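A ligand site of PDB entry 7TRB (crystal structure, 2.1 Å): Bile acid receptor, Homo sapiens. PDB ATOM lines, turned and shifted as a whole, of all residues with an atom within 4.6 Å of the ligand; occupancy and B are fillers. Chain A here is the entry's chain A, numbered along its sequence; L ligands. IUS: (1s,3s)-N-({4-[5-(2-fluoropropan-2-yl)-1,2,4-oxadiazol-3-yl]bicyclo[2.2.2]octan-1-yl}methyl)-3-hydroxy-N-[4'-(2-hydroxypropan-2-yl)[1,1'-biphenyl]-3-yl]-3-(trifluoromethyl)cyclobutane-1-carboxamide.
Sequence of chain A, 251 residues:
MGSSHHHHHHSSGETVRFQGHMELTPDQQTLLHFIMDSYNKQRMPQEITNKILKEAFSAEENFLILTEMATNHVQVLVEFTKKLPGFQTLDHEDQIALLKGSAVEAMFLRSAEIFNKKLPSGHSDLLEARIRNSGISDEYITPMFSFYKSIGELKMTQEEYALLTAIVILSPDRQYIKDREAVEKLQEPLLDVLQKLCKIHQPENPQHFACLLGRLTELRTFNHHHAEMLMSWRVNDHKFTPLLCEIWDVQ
A ring nitrogen (NE2) of His 73 lies within hydrogen-bond range of an oxygen (O2) of the ligand (2.6 Å). An oxygen (O4) of the ligand is in hydrogen-bond range of the side-chain amide oxygen of Asn 62 (3.2 Å).
Merely in contact with the ligand: Thr 49, Ile 52, Ile 65, Leu 66, Thr 67, Met 69, Ala 70, Met 107, Ser 111, Ile 114, Phe 115, Leu 119, Leu 127, Arg 130, Ile 131, Tyr 140, Met 144, Phe 145, Tyr 148, His 226, Met 229, Leu 230, Trp 233, Leu 244 and Trp 248. Hydrophobic or aromatic side chains within 4 Å of the ligand: Ile 52, Ile 65, Leu 66, Met 69, Ala 70, His 73, Met 107, Ile 114, Phe 115, Leu 119, Ile 131, Met 144, Phe 145, Tyr 148, His 226, Met 229, Leu 230, Trp 233, Leu 244 and Trp 248.
The side-chain hydroxyl (OG) of Ser 111 lies within hydrogen-bond range of the backbone carbonyl oxygen (O) of Met 107 (2.9 Å). The side-chain hydroxyl of Ser 111 sits at hydrogen-bond distance from the backbone carbonyl oxygen of Phe 108 (3.1 Å). OH of Tyr 140 is in hydrogen-bond range of ND1 of His 226, at 2.7 Å. The backbone carbonyl oxygen (O) of Ile 114 is in hydrogen-bond range of the backbone NH (N) of Leu 119 (2.8 Å). OH of Tyr 148 sits at hydrogen-bond distance from OG of Ser 111, at 3.0 Å. The side-chain hydroxyl of Ser 134 sits at hydrogen-bond distance from the backbone carbonyl oxygen of Ile 131 (2.7 Å).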
ATOM      1  N   THR A  49     -20.535  35.392  -3.417  1.00  0.00           N
ATOM      2  CA  THR A  49     -20.698  35.436  -1.962  1.00  0.00           C
ATOM      3  C   THR A  49     -21.773  36.441  -1.509  1.00  0.00           C
ATOM      4  O   THR A  49     -22.658  36.087  -0.732  1.00  0.00           O
ATOM      5  CB  THR A  49     -19.338  35.678  -1.288  1.00  0.00           C
ATOM      6  N   ILE A  52     -25.452  35.640  -2.827  1.00  0.00           N
ATOM      7  CA  ILE A  52     -26.025  34.468  -2.157  1.00  0.00           C
ATOM      8  C   ILE A  52     -26.938  34.847  -0.993  1.00  0.00           C
ATOM      9  O   ILE A  52     -28.098  34.446  -0.976  1.00  0.00           O
ATOM     10  CB  ILE A  52     -24.921  33.481  -1.703  1.00  0.00           C
ATOM     11  N   PHE A  57     -32.906  34.861  -4.793  1.00  0.00           N
ATOM     12  CA  PHE A  57     -32.924  33.863  -5.867  1.00  0.00           C
ATOM     13  C   PHE A  57     -34.267  33.096  -5.949  1.00  0.00           C
ATOM     14  O   PHE A  57     -34.990  33.001  -4.947  1.00  0.00           O
ATOM     15  CB  PHE A  57     -31.726  32.905  -5.752  1.00  0.00           C
ATOM     16  N   ASN A  62     -32.216  27.965  -7.552  1.00  0.00           N
ATOM     17  CA  ASN A  62     -31.619  27.604  -6.264  1.00  0.00           C
ATOM     18  C   ASN A  62     -30.883  26.262  -6.375  1.00  0.00           C
ATOM     19  O   ASN A  62     -29.715  26.193  -5.977  1.00  0.00           O
ATOM     20  CB  ASN A  62     -32.712  27.497  -5.176  1.00  0.00           C
ATOM     21  CG  ASN A  62     -33.076  28.785  -4.469  1.00  0.00           C
ATOM     22  OD1 ASN A  62     -32.393  29.816  -4.570  1.00  0.00           O
ATOM     23  ND2 ASN A  62     -34.188  28.759  -3.762  1.00  0.00           N
ATOM     24  N   ILE A  65     -27.626  26.803  -8.354  1.00  0.00           N
ATOM     25  CA  ILE A  65     -26.586  27.505  -7.582  1.00  0.00           C
ATOM     26  C   ILE A  65     -25.881  26.511  -6.644  1.00  0.00           C
ATOM     27  O   ILE A  65     -24.648  26.528  -6.542  1.00  0.00           O
ATOM     28  CB  ILE A  65     -27.160  28.733  -6.801  1.00  0.00           C
ATOM     29  CG1 ILE A  65     -27.772  29.780  -7.755  1.00  0.00           C
ATOM     30  CG2 ILE A  65     -26.095  29.396  -5.888  1.00  0.00           C
ATOM     31  CD1 ILE A  65     -28.870  30.673  -7.108  1.00  0.00           C
ATOM     32  N   LEU A  66     -26.679  25.642  -5.960  1.00  0.00           N
ATOM     33  CA  LEU A  66     -26.182  24.612  -5.039  1.00  0.00           C
ATOM     34  C   LEU A  66     -25.280  23.627  -5.765  1.00  0.00           C
ATOM     35  O   LEU A  66     -24.252  23.234  -5.198  1.00  0.00           O
ATOM     36  CB  LEU A  66     -27.338  23.863  -4.354  1.00  0.00           C
ATOM     37  CG  LEU A  66     -28.195  24.640  -3.361  1.00  0.00           C
ATOM     38  CD1 LEU A  66     -29.357  23.811  -2.911  1.00  0.00           C
ATOM     39  CD2 LEU A  66     -27.412  25.100  -2.151  1.00  0.00           C
ATOM     40  N   THR A  67     -25.636  23.239  -7.004  1.00  0.00           N
ATOM     41  CA  THR A  67     -24.825  22.321  -7.818  1.00  0.00           C
ATOM     42  C   THR A  67     -23.516  23.020  -8.253  1.00  0.00           C
ATOM     43  O   THR A  67     -22.499  22.353  -8.354  1.00  0.00           O
ATOM     44  CB  THR A  67     -25.649  21.712  -8.960  1.00  0.00           C
ATOM     45  OG1 THR A  67     -26.889  21.237  -8.424  1.00  0.00           O
ATOM     46  CG2 THR A  67     -24.950  20.541  -9.622  1.00  0.00           C
ATOM     47  N   MET A  69     -21.973  25.579  -6.416  1.00  0.00           N
ATOM     48  CA  MET A  69     -21.279  25.717  -5.123  1.00  0.00           C
ATOM     49  C   MET A  69     -20.489  24.476  -4.785  1.00  0.00           C
ATOM     50  O   MET A  69     -19.292  24.574  -4.507  1.00  0.00           O
ATOM     51  CB  MET A  69     -22.269  25.961  -3.994  1.00  0.00           C
ATOM     52  CG  MET A  69     -22.635  27.378  -3.830  1.00  0.00           C
ATOM     53  SD  MET A  69     -24.011  27.491  -2.695  1.00  0.00           S
ATOM     54  CE  MET A  69     -24.210  29.292  -2.638  1.00  0.00           C
ATOM     55  N   ALA A  70     -21.155  23.309  -4.838  1.00  0.00           N
ATOM     56  CA  ALA A  70     -20.579  22.020  -4.544  1.00  0.00           C
ATOM     57  C   ALA A  70     -19.437  21.657  -5.494  1.00  0.00           C
ATOM     58  O   ALA A  70     -18.415  21.164  -5.047  1.00  0.00           O
ATOM     59  CB  ALA A  70     -21.668  20.960  -4.564  1.00  0.00           C
ATOM     60  N   HIS A  73     -16.345  23.765  -4.638  1.00  0.00           N
ATOM     61  CA  HIS A  73     -15.715  23.231  -3.436  1.00  0.00           C
ATOM     62  C   HIS A  73     -14.812  22.077  -3.841  1.00  0.00           C
ATOM     63  O   HIS A  73     -13.632  22.043  -3.470  1.00  0.00           O
ATOM     64  CB  HIS A  73     -16.788  22.706  -2.469  1.00  0.00           C
ATOM     65  CG  HIS A  73     -17.339  23.760  -1.550  1.00  0.00           C
ATOM     66  ND1 HIS A  73     -16.608  24.233  -0.463  1.00  0.00           N
ATOM     67  CD2 HIS A  73     -18.553  24.353  -1.552  1.00  0.00           C
ATOM     68  CE1 HIS A  73     -17.379  25.130   0.119  1.00  0.00           C
ATOM     69  NE2 HIS A  73     -18.561  25.231  -0.494  1.00  0.00           N
ATOM     70  N   MET A 107     -15.351  20.344   2.574  1.00  0.00           N
ATOM     71  CA  MET A 107     -16.359  21.293   2.094  1.00  0.00           C
ATOM     72  C   MET A 107     -17.020  22.016   3.281  1.00  0.00           C
ATOM     73  O   MET A 107     -17.098  23.245   3.239  1.00  0.00           O
ATOM     74  CB  MET A 107     -17.382  20.584   1.193  1.00  0.00           C
ATOM     75  CG  MET A 107     -18.552  21.450   0.793  1.00  0.00           C
ATOM     76  SD  MET A 107     -19.586  20.661  -0.451  1.00  0.00           S
ATOM     77  CE  MET A 107     -20.271  19.238   0.487  1.00  0.00           C
ATOM     78  N   PHE A 108     -17.467  21.279   4.341  1.00  0.00           N
ATOM     79  CA  PHE A 108     -18.093  21.908   5.524  1.00  0.00           C
ATOM     80  C   PHE A 108     -17.126  22.772   6.325  1.00  0.00           C
ATOM     81  O   PHE A 108     -17.514  23.815   6.853  1.00  0.00           O
ATOM     82  CB  PHE A 108     -18.817  20.890   6.421  1.00  0.00           C
ATOM     83  CG  PHE A 108     -20.139  20.465   5.847  1.00  0.00           C
ATOM     84  CD1 PHE A 108     -20.240  19.342   5.035  1.00  0.00           C
ATOM     85  CD2 PHE A 108     -21.290  21.218   6.069  1.00  0.00           C
ATOM     86  CE1 PHE A 108     -21.447  18.964   4.471  1.00  0.00           C
ATOM     87  CE2 PHE A 108     -22.504  20.845   5.500  1.00  0.00           C
ATOM     88  CZ  PHE A 108     -22.577  19.719   4.728  1.00  0.00           C
ATOM     89  N   SER A 111     -16.516  26.072   4.235  1.00  0.00           N
ATOM     90  CA  SER A 111     -17.670  26.967   4.318  1.00  0.00           C
ATOM     91  C   SER A 111     -17.729  27.651   5.667  1.00  0.00           C
ATOM     92  O   SER A 111     -18.144  28.812   5.730  1.00  0.00           O
ATOM     93  CB  SER A 111     -18.980  26.259   3.967  1.00  0.00           C
ATOM     94  OG  SER A 111     -19.062  24.934   4.458  1.00  0.00           O
ATOM     95  N   ILE A 114     -15.401  30.744   5.677  1.00  0.00           N
ATOM     96  CA  ILE A 114     -16.023  31.887   5.008  1.00  0.00           C
ATOM     97  C   ILE A 114     -17.086  32.518   5.926  1.00  0.00           C
ATOM     98  O   ILE A 114     -17.025  33.718   6.207  1.00  0.00           O
ATOM     99  CB  ILE A 114     -16.577  31.498   3.608  1.00  0.00           C
ATOM    100  CG1 ILE A 114     -15.490  30.835   2.727  1.00  0.00           C
ATOM    101  CG2 ILE A 114     -17.188  32.719   2.889  1.00  0.00           C
ATOM    102  CD1 ILE A 114     -16.002  29.952   1.565  1.00  0.00           C
ATOM    103  N   PHE A 115     -18.023  31.675   6.425  1.00  0.00           N
ATOM    104  CA  PHE A 115     -19.149  32.016   7.302  1.00  0.00           C
ATOM    105  C   PHE A 115     -18.789  32.765   8.583  1.00  0.00           C
ATOM    106  O   PHE A 115     -19.580  33.584   9.071  1.00  0.00           O
ATOM    107  CB  PHE A 115     -19.918  30.748   7.662  1.00  0.00           C
ATOM    108  CG  PHE A 115     -21.258  30.689   6.990  1.00  0.00           C
ATOM    109  CD1 PHE A 115     -21.370  30.402   5.639  1.00  0.00           C
ATOM    110  CD2 PHE A 115     -22.426  30.960   7.704  1.00  0.00           C
ATOM    111  CE1 PHE A 115     -22.609  30.412   5.003  1.00  0.00           C
ATOM    112  CE2 PHE A 115     -23.662  30.956   7.070  1.00  0.00           C
ATOM    113  CZ  PHE A 115     -23.746  30.677   5.724  1.00  0.00           C
ATOM    114  N   LEU A 119     -17.279  36.495   5.909  1.00  0.00           N
ATOM    115  CA  LEU A 119     -18.619  37.084   6.008  1.00  0.00           C
ATOM    116  C   LEU A 119     -18.955  37.530   7.448  1.00  0.00           C
ATOM    117  O   LEU A 119     -18.685  36.790   8.393  1.00  0.00           O
ATOM    118  CB  LEU A 119     -19.653  36.066   5.501  1.00  0.00           C
ATOM    119  CG  LEU A 119     -20.137  36.200   4.068  1.00  0.00           C
ATOM    120  CD1 LEU A 119     -18.998  36.130   3.050  1.00  0.00           C
ATOM    121  CD2 LEU A 119     -21.159  35.124   3.751  1.00  0.00           C
ATOM    122  N   LEU A 127     -28.232  34.120   5.019  1.00  0.00           N
ATOM    123  CA  LEU A 127     -27.863  32.927   4.247  1.00  0.00           C
ATOM    124  C   LEU A 127     -28.545  31.667   4.762  1.00  0.00           C
ATOM    125  O   LEU A 127     -28.866  30.784   3.976  1.00  0.00           O
ATOM    126  CB  LEU A 127     -26.332  32.745   4.207  1.00  0.00           C
ATOM    127  N   ARG A 130     -32.327  32.002   3.733  1.00  0.00           N
ATOM    128  CA  ARG A 130     -32.401  31.766   2.301  1.00  0.00           C
ATOM    129  C   ARG A 130     -32.294  30.265   1.928  1.00  0.00           C
ATOM    130  O   ARG A 130     -33.063  29.809   1.085  1.00  0.00           O
ATOM    131  CB  ARG A 130     -31.372  32.613   1.555  1.00  0.00           C
ATOM    132  N   ILE A 131     -31.365  29.518   2.583  1.00  0.00           N
ATOM    133  CA  ILE A 131     -31.143  28.088   2.336  1.00  0.00           C
ATOM    134  C   ILE A 131     -32.315  27.248   2.884  1.00  0.00           C
ATOM    135  O   ILE A 131     -32.689  26.242   2.262  1.00  0.00           O
ATOM    136  CB  ILE A 131     -29.728  27.582   2.791  1.00  0.00           C
ATOM    137  CG1 ILE A 131     -29.382  26.213   2.119  1.00  0.00           C
ATOM    138  CG2 ILE A 131     -29.550  27.542   4.314  1.00  0.00           C
ATOM    139  CD1 ILE A 131     -27.985  25.698   2.274  1.00  0.00           C
ATOM    140  N   SER A 134     -35.578  27.332   0.720  1.00  0.00           N
ATOM    141  CA  SER A 134     -35.339  26.560  -0.492  1.00  0.00           C
ATOM    142  C   SER A 134     -35.829  25.127  -0.204  1.00  0.00           C
ATOM    143  O   SER A 134     -36.529  24.898   0.798  1.00  0.00           O
ATOM    144  CB  SER A 134     -33.868  26.607  -0.888  1.00  0.00           C
ATOM    145  OG  SER A 134     -33.072  25.561  -0.325  1.00  0.00           O
ATOM    146  N   ILE A 136     -34.035  22.027   0.461  1.00  0.00           N
ATOM    147  CA  ILE A 136     -33.222  21.288   1.442  1.00  0.00           C
ATOM    148  C   ILE A 136     -33.892  21.130   2.832  1.00  0.00           C
ATOM    149  O   ILE A 136     -34.501  22.055   3.369  1.00  0.00           O
ATOM    150  CB  ILE A 136     -31.781  21.873   1.567  1.00  0.00           C
ATOM    151  CG1 ILE A 136     -31.131  22.203   0.167  1.00  0.00           C
ATOM    152  CG2 ILE A 136     -30.867  20.957   2.407  1.00  0.00           C
ATOM    153  CD1 ILE A 136     -30.292  21.068  -0.609  1.00  0.00           C
ATOM    154  N   TYR A 140     -30.751  18.455   7.527  1.00  0.00           N
ATOM    155  CA  TYR A 140     -29.474  18.805   6.931  1.00  0.00           C
ATOM    156  C   TYR A 140     -28.998  20.194   7.397  1.00  0.00           C
ATOM    157  O   TYR A 140     -27.838  20.308   7.803  1.00  0.00           O
ATOM    158  CB  TYR A 140     -29.587  18.728   5.397  1.00  0.00           C
ATOM    159  CG  TYR A 140     -28.259  18.772   4.675  1.00  0.00           C
ATOM    160  CD1 TYR A 140     -27.458  17.635   4.581  1.00  0.00           C
ATOM    161  CD2 TYR A 140     -27.827  19.937   4.061  1.00  0.00           C
ATOM    162  CE1 TYR A 140     -26.242  17.671   3.910  1.00  0.00           C
ATOM    163  CE2 TYR A 140     -26.628  19.979   3.357  1.00  0.00           C
ATOM    164  CZ  TYR A 140     -25.832  18.854   3.307  1.00  0.00           C
ATOM    165  OH  TYR A 140     -24.635  18.913   2.626  1.00  0.00           O
ATOM    166  N   MET A 144     -25.781  21.638  10.223  1.00  0.00           N
ATOM    167  CA  MET A 144     -24.890  22.494   9.432  1.00  0.00           C
ATOM    168  C   MET A 144     -24.585  23.813  10.145  1.00  0.00           C
ATOM    169  O   MET A 144     -23.423  24.198  10.267  1.00  0.00           O
ATOM    170  CB  MET A 144     -25.482  22.737   8.029  1.00  0.00           C
ATOM    171  CG  MET A 144     -24.632  23.698   7.170  1.00  0.00           C
ATOM    172  SD  MET A 144     -25.332  24.141   5.557  1.00  0.00           S
ATOM    173  CE  MET A 144     -25.465  22.599   4.872  1.00  0.00           C
ATOM    174  N   PHE A 145     -25.630  24.498  10.634  1.00  0.00           N
ATOM    175  CA  PHE A 145     -25.509  25.758  11.332  1.00  0.00           C
ATOM    176  C   PHE A 145     -25.101  25.598  12.780  1.00  0.00           C
ATOM    177  O   PHE A 145     -24.472  26.507  13.328  1.00  0.00           O
ATOM    178  CB  PHE A 145     -26.768  26.584  11.181  1.00  0.00           C
ATOM    179  CG  PHE A 145     -26.776  27.239   9.821  1.00  0.00           C
ATOM    180  CD1 PHE A 145     -26.140  28.466   9.626  1.00  0.00           C
ATOM    181  CD2 PHE A 145     -27.358  26.620   8.725  1.00  0.00           C
ATOM    182  CE1 PHE A 145     -26.115  29.055   8.366  1.00  0.00           C
ATOM    183  CE2 PHE A 145     -27.337  27.209   7.474  1.00  0.00           C
ATOM    184  CZ  PHE A 145     -26.708  28.422   7.298  1.00  0.00           C
ATOM    185  N   TYR A 148     -21.380  25.474  12.378  1.00  0.00           N
ATOM    186  CA  TYR A 148     -20.894  26.843  12.121  1.00  0.00           C
ATOM    187  C   TYR A 148     -20.842  27.716  13.387  1.00  0.00           C
ATOM    188  O   TYR A 148     -19.884  28.502  13.547  1.00  0.00           O
ATOM    189  CB  TYR A 148     -21.768  27.535  11.081  1.00  0.00           C
ATOM    190  CG  TYR A 148     -21.735  26.997   9.661  1.00  0.00           C
ATOM    191  CD1 TYR A 148     -20.735  26.118   9.246  1.00  0.00           C
ATOM    192  CD2 TYR A 148     -22.680  27.397   8.726  1.00  0.00           C
ATOM    193  CE1 TYR A 148     -20.707  25.625   7.951  1.00  0.00           C
ATOM    194  CE2 TYR A 148     -22.672  26.891   7.431  1.00  0.00           C
ATOM    195  CZ  TYR A 148     -21.679  26.007   7.047  1.00  0.00           C
ATOM    196  OH  TYR A 148     -21.691  25.556   5.752  1.00  0.00           O
ATOM    197  N   HIS A 226     -24.888  14.119   4.396  1.00  0.00           N
ATOM    198  CA  HIS A 226     -24.725  14.450   2.980  1.00  0.00           C
ATOM    199  C   HIS A 226     -25.250  13.337   2.097  1.00  0.00           C
ATOM    200  O   HIS A 226     -26.008  13.620   1.189  1.00  0.00           O
ATOM    201  CB  HIS A 226     -23.265  14.827   2.640  1.00  0.00           C
ATOM    202  CG  HIS A 226     -23.133  15.540   1.328  1.00  0.00           C
ATOM    203  ND1 HIS A 226     -23.559  16.846   1.178  1.00  0.00           N
ATOM    204  CD2 HIS A 226     -22.699  15.081   0.140  1.00  0.00           C
ATOM    205  CE1 HIS A 226     -23.330  17.149  -0.084  1.00  0.00           C
ATOM    206  NE2 HIS A 226     -22.834  16.117  -0.746  1.00  0.00           N
ATOM    207  N   MET A 229     -29.005  13.471   1.948  1.00  0.00           N
ATOM    208  CA  MET A 229     -29.329  14.608   1.093  1.00  0.00           C
ATOM    209  C   MET A 229     -29.145  14.247  -0.400  1.00  0.00           C
ATOM    210  O   MET A 229     -29.935  14.695  -1.232  1.00  0.00           O
ATOM    211  CB  MET A 229     -28.480  15.811   1.529  1.00  0.00           C
ATOM    212  CG  MET A 229     -28.929  17.118   0.963  1.00  0.00           C
ATOM    213  SD  MET A 229     -28.035  17.548  -0.549  1.00  0.00           S
ATOM    214  CE  MET A 229     -26.641  18.313   0.106  1.00  0.00           C
ATOM    215  N   LEU A 230     -28.171  13.389  -0.724  1.00  0.00           N
ATOM    216  CA  LEU A 230     -27.881  12.969  -2.099  1.00  0.00           C
ATOM    217  C   LEU A 230     -28.956  12.034  -2.674  1.00  0.00           C
ATOM    218  O   LEU A 230     -29.289  12.177  -3.859  1.00  0.00           O
ATOM    219  CB  LEU A 230     -26.495  12.312  -2.194  1.00  0.00           C
ATOM    220  CG  LEU A 230     -25.238  13.170  -1.930  1.00  0.00           C
ATOM    221  CD1 LEU A 230     -23.998  12.283  -1.813  1.00  0.00           C
ATOM    222  CD2 LEU A 230     -25.031  14.229  -2.976  1.00  0.00           C
ATOM    223  N   TRP A 233     -31.876  14.120  -3.541  1.00  0.00           N
ATOM    224  CA  TRP A 233     -31.536  14.955  -4.697  1.00  0.00           C
ATOM    225  C   TRP A 233     -31.878  14.256  -6.024  1.00  0.00           C
ATOM    226  O   TRP A 233     -32.484  14.889  -6.887  1.00  0.00           O
ATOM    227  CB  TRP A 233     -30.031  15.303  -4.642  1.00  0.00           C
ATOM    228  CG  TRP A 233     -29.614  16.552  -5.368  1.00  0.00           C
ATOM    229  CD1 TRP A 233     -28.850  16.639  -6.496  1.00  0.00           C
ATOM    230  CD2 TRP A 233     -29.891  17.908  -4.969  1.00  0.00           C
ATOM    231  NE1 TRP A 233     -28.641  17.954  -6.833  1.00  0.00           N
ATOM    232  CE2 TRP A 233     -29.261  18.754  -5.910  1.00  0.00           C
ATOM    233  CE3 TRP A 233     -30.605  18.474  -3.907  1.00  0.00           C
ATOM    234  CZ2 TRP A 233     -29.356  20.151  -5.833  1.00  0.00           C
ATOM    235  CZ3 TRP A 233     -30.688  19.852  -3.823  1.00  0.00           C
ATOM    236  CH2 TRP A 233     -30.061  20.681  -4.778  1.00  0.00           C
ATOM    237  N   PHE A 240     -27.005  16.435 -11.416  1.00  0.00           N
ATOM    238  CA  PHE A 240     -25.655  16.228 -10.868  1.00  0.00           C
ATOM    239  C   PHE A 240     -24.655  16.400 -11.998  1.00  0.00           C
ATOM    240  O   PHE A 240     -24.872  15.877 -13.101  1.00  0.00           O
ATOM    241  CB  PHE A 240     -25.464  14.810 -10.290  1.00  0.00           C
ATOM    242  CG  PHE A 240     -25.940  14.579  -8.882  1.00  0.00           C
ATOM    243  CD1 PHE A 240     -25.260  15.134  -7.800  1.00  0.00           C
ATOM    244  CD2 PHE A 240     -27.024  13.759  -8.630  1.00  0.00           C
ATOM    245  CE1 PHE A 240     -25.688  14.901  -6.502  1.00  0.00           C
ATOM    246  CE2 PHE A 240     -27.443  13.512  -7.338  1.00  0.00           C
ATOM    247  CZ  PHE A 240     -26.772  14.090  -6.284  1.00  0.00           C
ATOM    248  N   LEU A 244     -19.310  15.761  -9.526  1.00  0.00           N
ATOM    249  CA  LEU A 244     -20.056  15.371  -8.321  1.00  0.00           C
ATOM    250  C   LEU A 244     -20.397  13.874  -8.295  1.00  0.00           C
ATOM    251  O   LEU A 244     -20.300  13.260  -7.229  1.00  0.00           O
ATOM    252  CB  LEU A 244     -21.320  16.220  -8.141  1.00  0.00           C
ATOM    253  CG  LEU A 244     -21.084  17.727  -7.905  1.00  0.00           C
ATOM    254  CD1 LEU A 244     -22.390  18.451  -7.693  1.00  0.00           C
ATOM    255  CD2 LEU A 244     -20.131  17.965  -6.750  1.00  0.00           C
ATOM    256  N   TRP A 248     -18.604  11.283  -5.383  1.00  0.00           N
ATOM    257  CA  TRP A 248     -19.558  10.729  -4.428  1.00  0.00           C
ATOM    258  C   TRP A 248     -20.297   9.444  -4.871  1.00  0.00           C
ATOM    259  O   TRP A 248     -21.100   8.927  -4.094  1.00  0.00           O
ATOM    260  CB  TRP A 248     -20.578  11.810  -4.011  1.00  0.00           C
ATOM    261  CG  TRP A 248     -19.965  12.900  -3.192  1.00  0.00           C
ATOM    262  CD1 TRP A 248     -19.013  12.750  -2.228  1.00  0.00           C
ATOM    263  CD2 TRP A 248     -20.281  14.286  -3.242  1.00  0.00           C
ATOM    264  NE1 TRP A 248     -18.678  13.983  -1.706  1.00  0.00           N
ATOM    265  CE2 TRP A 248     -19.453  14.935  -2.293  1.00  0.00           C
ATOM    266  CE3 TRP A 248     -21.205  15.052  -3.976  1.00  0.00           C
ATOM    267  CZ2 TRP A 248     -19.524  16.309  -2.052  1.00  0.00           C
ATOM    268  CZ3 TRP A 248     -21.264  16.421  -3.738  1.00  0.00           C
ATOM    269  CH2 TRP A 248     -20.420  17.030  -2.792  1.00  0.00           C
HETATM  270  C13 IUS L   1     -24.199  22.342  -0.372  1.00  0.00           C
HETATM  271  C18 IUS L   1     -25.161  19.937  -2.784  1.00  0.00           C
HETATM  272  C17 IUS L   1     -24.886  21.390  -1.324  1.00  0.00           C
HETATM  273  C16 IUS L   1     -22.726  24.394  -0.268  1.00  0.00           C
HETATM  274  C15 IUS L   1     -23.428  23.397  -1.196  1.00  0.00           C
HETATM  275  C19 IUS L   1     -25.115  18.907  -3.891  1.00  0.00           C
HETATM  276  C20 IUS L   1     -26.128  17.782  -3.682  1.00  0.00           C
HETATM  277  C21 IUS L   1     -25.412  19.607  -5.221  1.00  0.00           C
HETATM  278  C22 IUS L   1     -26.871  28.281  -0.401  1.00  0.00           C
HETATM  279  C23 IUS L   1     -27.815  28.747  -1.288  1.00  0.00           C
HETATM  280  C24 IUS L   1     -28.543  29.906  -1.024  1.00  0.00           C
HETATM  281  C11 IUS L   1     -24.537  24.091   1.407  1.00  0.00           C
HETATM  282  C12 IUS L   1     -25.232  23.057   0.518  1.00  0.00           C
HETATM  283  C34 IUS L   1     -31.003  29.864  -1.455  1.00  0.00           C
HETATM  284  C27 IUS L   1     -21.385  27.067   1.130  1.00  0.00           C
HETATM  285  C33 IUS L   1     -29.684  31.884  -2.122  1.00  0.00           C
HETATM  286  C1  IUS L   1     -24.479  27.760   1.347  1.00  0.00           C
HETATM  287  C2  IUS L   1     -25.643  28.400   1.790  1.00  0.00           C
HETATM  288  C3  IUS L   1     -25.878  28.479   3.158  1.00  0.00           C
HETATM  289  C4  IUS L   1     -24.987  27.951   4.071  1.00  0.00           C
HETATM  290  C5  IUS L   1     -23.827  27.333   3.636  1.00  0.00           C
HETATM  291  C6  IUS L   1     -23.582  27.214   2.275  1.00  0.00           C
HETATM  292  C7  IUS L   1     -26.607  28.949   0.800  1.00  0.00           C
HETATM  293  N1  IUS L   1     -22.425  26.503   1.815  1.00  0.00           N
HETATM  294  C8  IUS L   1     -23.190  21.632   0.549  1.00  0.00           C
HETATM  295  C9  IUS L   1     -22.518  22.638   1.494  1.00  0.00           C
HETATM  296  C10 IUS L   1     -23.021  24.065   1.197  1.00  0.00           C
HETATM  297  C14 IUS L   1     -22.341  25.066   2.146  1.00  0.00           C
HETATM  298  N2  IUS L   1     -24.212  20.464  -2.090  1.00  0.00           N
HETATM  299  O1  IUS L   1     -26.373  20.429  -2.509  1.00  0.00           O
HETATM  300  N3  IUS L   1     -26.171  21.421  -1.513  1.00  0.00           N
HETATM  301  F1  IUS L   1     -23.828  18.345  -3.962  1.00  0.00           F
HETATM  302  C25 IUS L   1     -28.272  30.587   0.158  1.00  0.00           C
HETATM  303  C26 IUS L   1     -27.321  30.117   1.049  1.00  0.00           C
HETATM  304  O2  IUS L   1     -20.380  26.434   0.883  1.00  0.00           O
HETATM  305  C28 IUS L   1     -21.487  28.528   0.742  1.00  0.00           C
HETATM  306  C29 IUS L   1     -20.411  30.342   1.214  1.00  0.00           C
HETATM  307  C30 IUS L   1     -21.473  29.519   1.929  1.00  0.00           C
HETATM  308  C31 IUS L   1     -20.209  29.212   0.208  1.00  0.00           C
HETATM  309  O3  IUS L   1     -19.284  30.549   2.076  1.00  0.00           O
HETATM  310  C32 IUS L   1     -29.666  30.368  -1.969  1.00  0.00           C
HETATM  311  O4  IUS L   1     -29.480  29.810  -3.289  1.00  0.00           O
HETATM  312  C35 IUS L   1     -20.828  31.706   0.677  1.00  0.00           C
HETATM  313  F2  IUS L   1     -20.518  32.695   1.505  1.00  0.00           F
HETATM  314  F3  IUS L   1     -22.135  31.787   0.465  1.00  0.00           F
HETATM  315  F4  IUS L   1     -20.237  31.986  -0.490  1.00  0.00           F
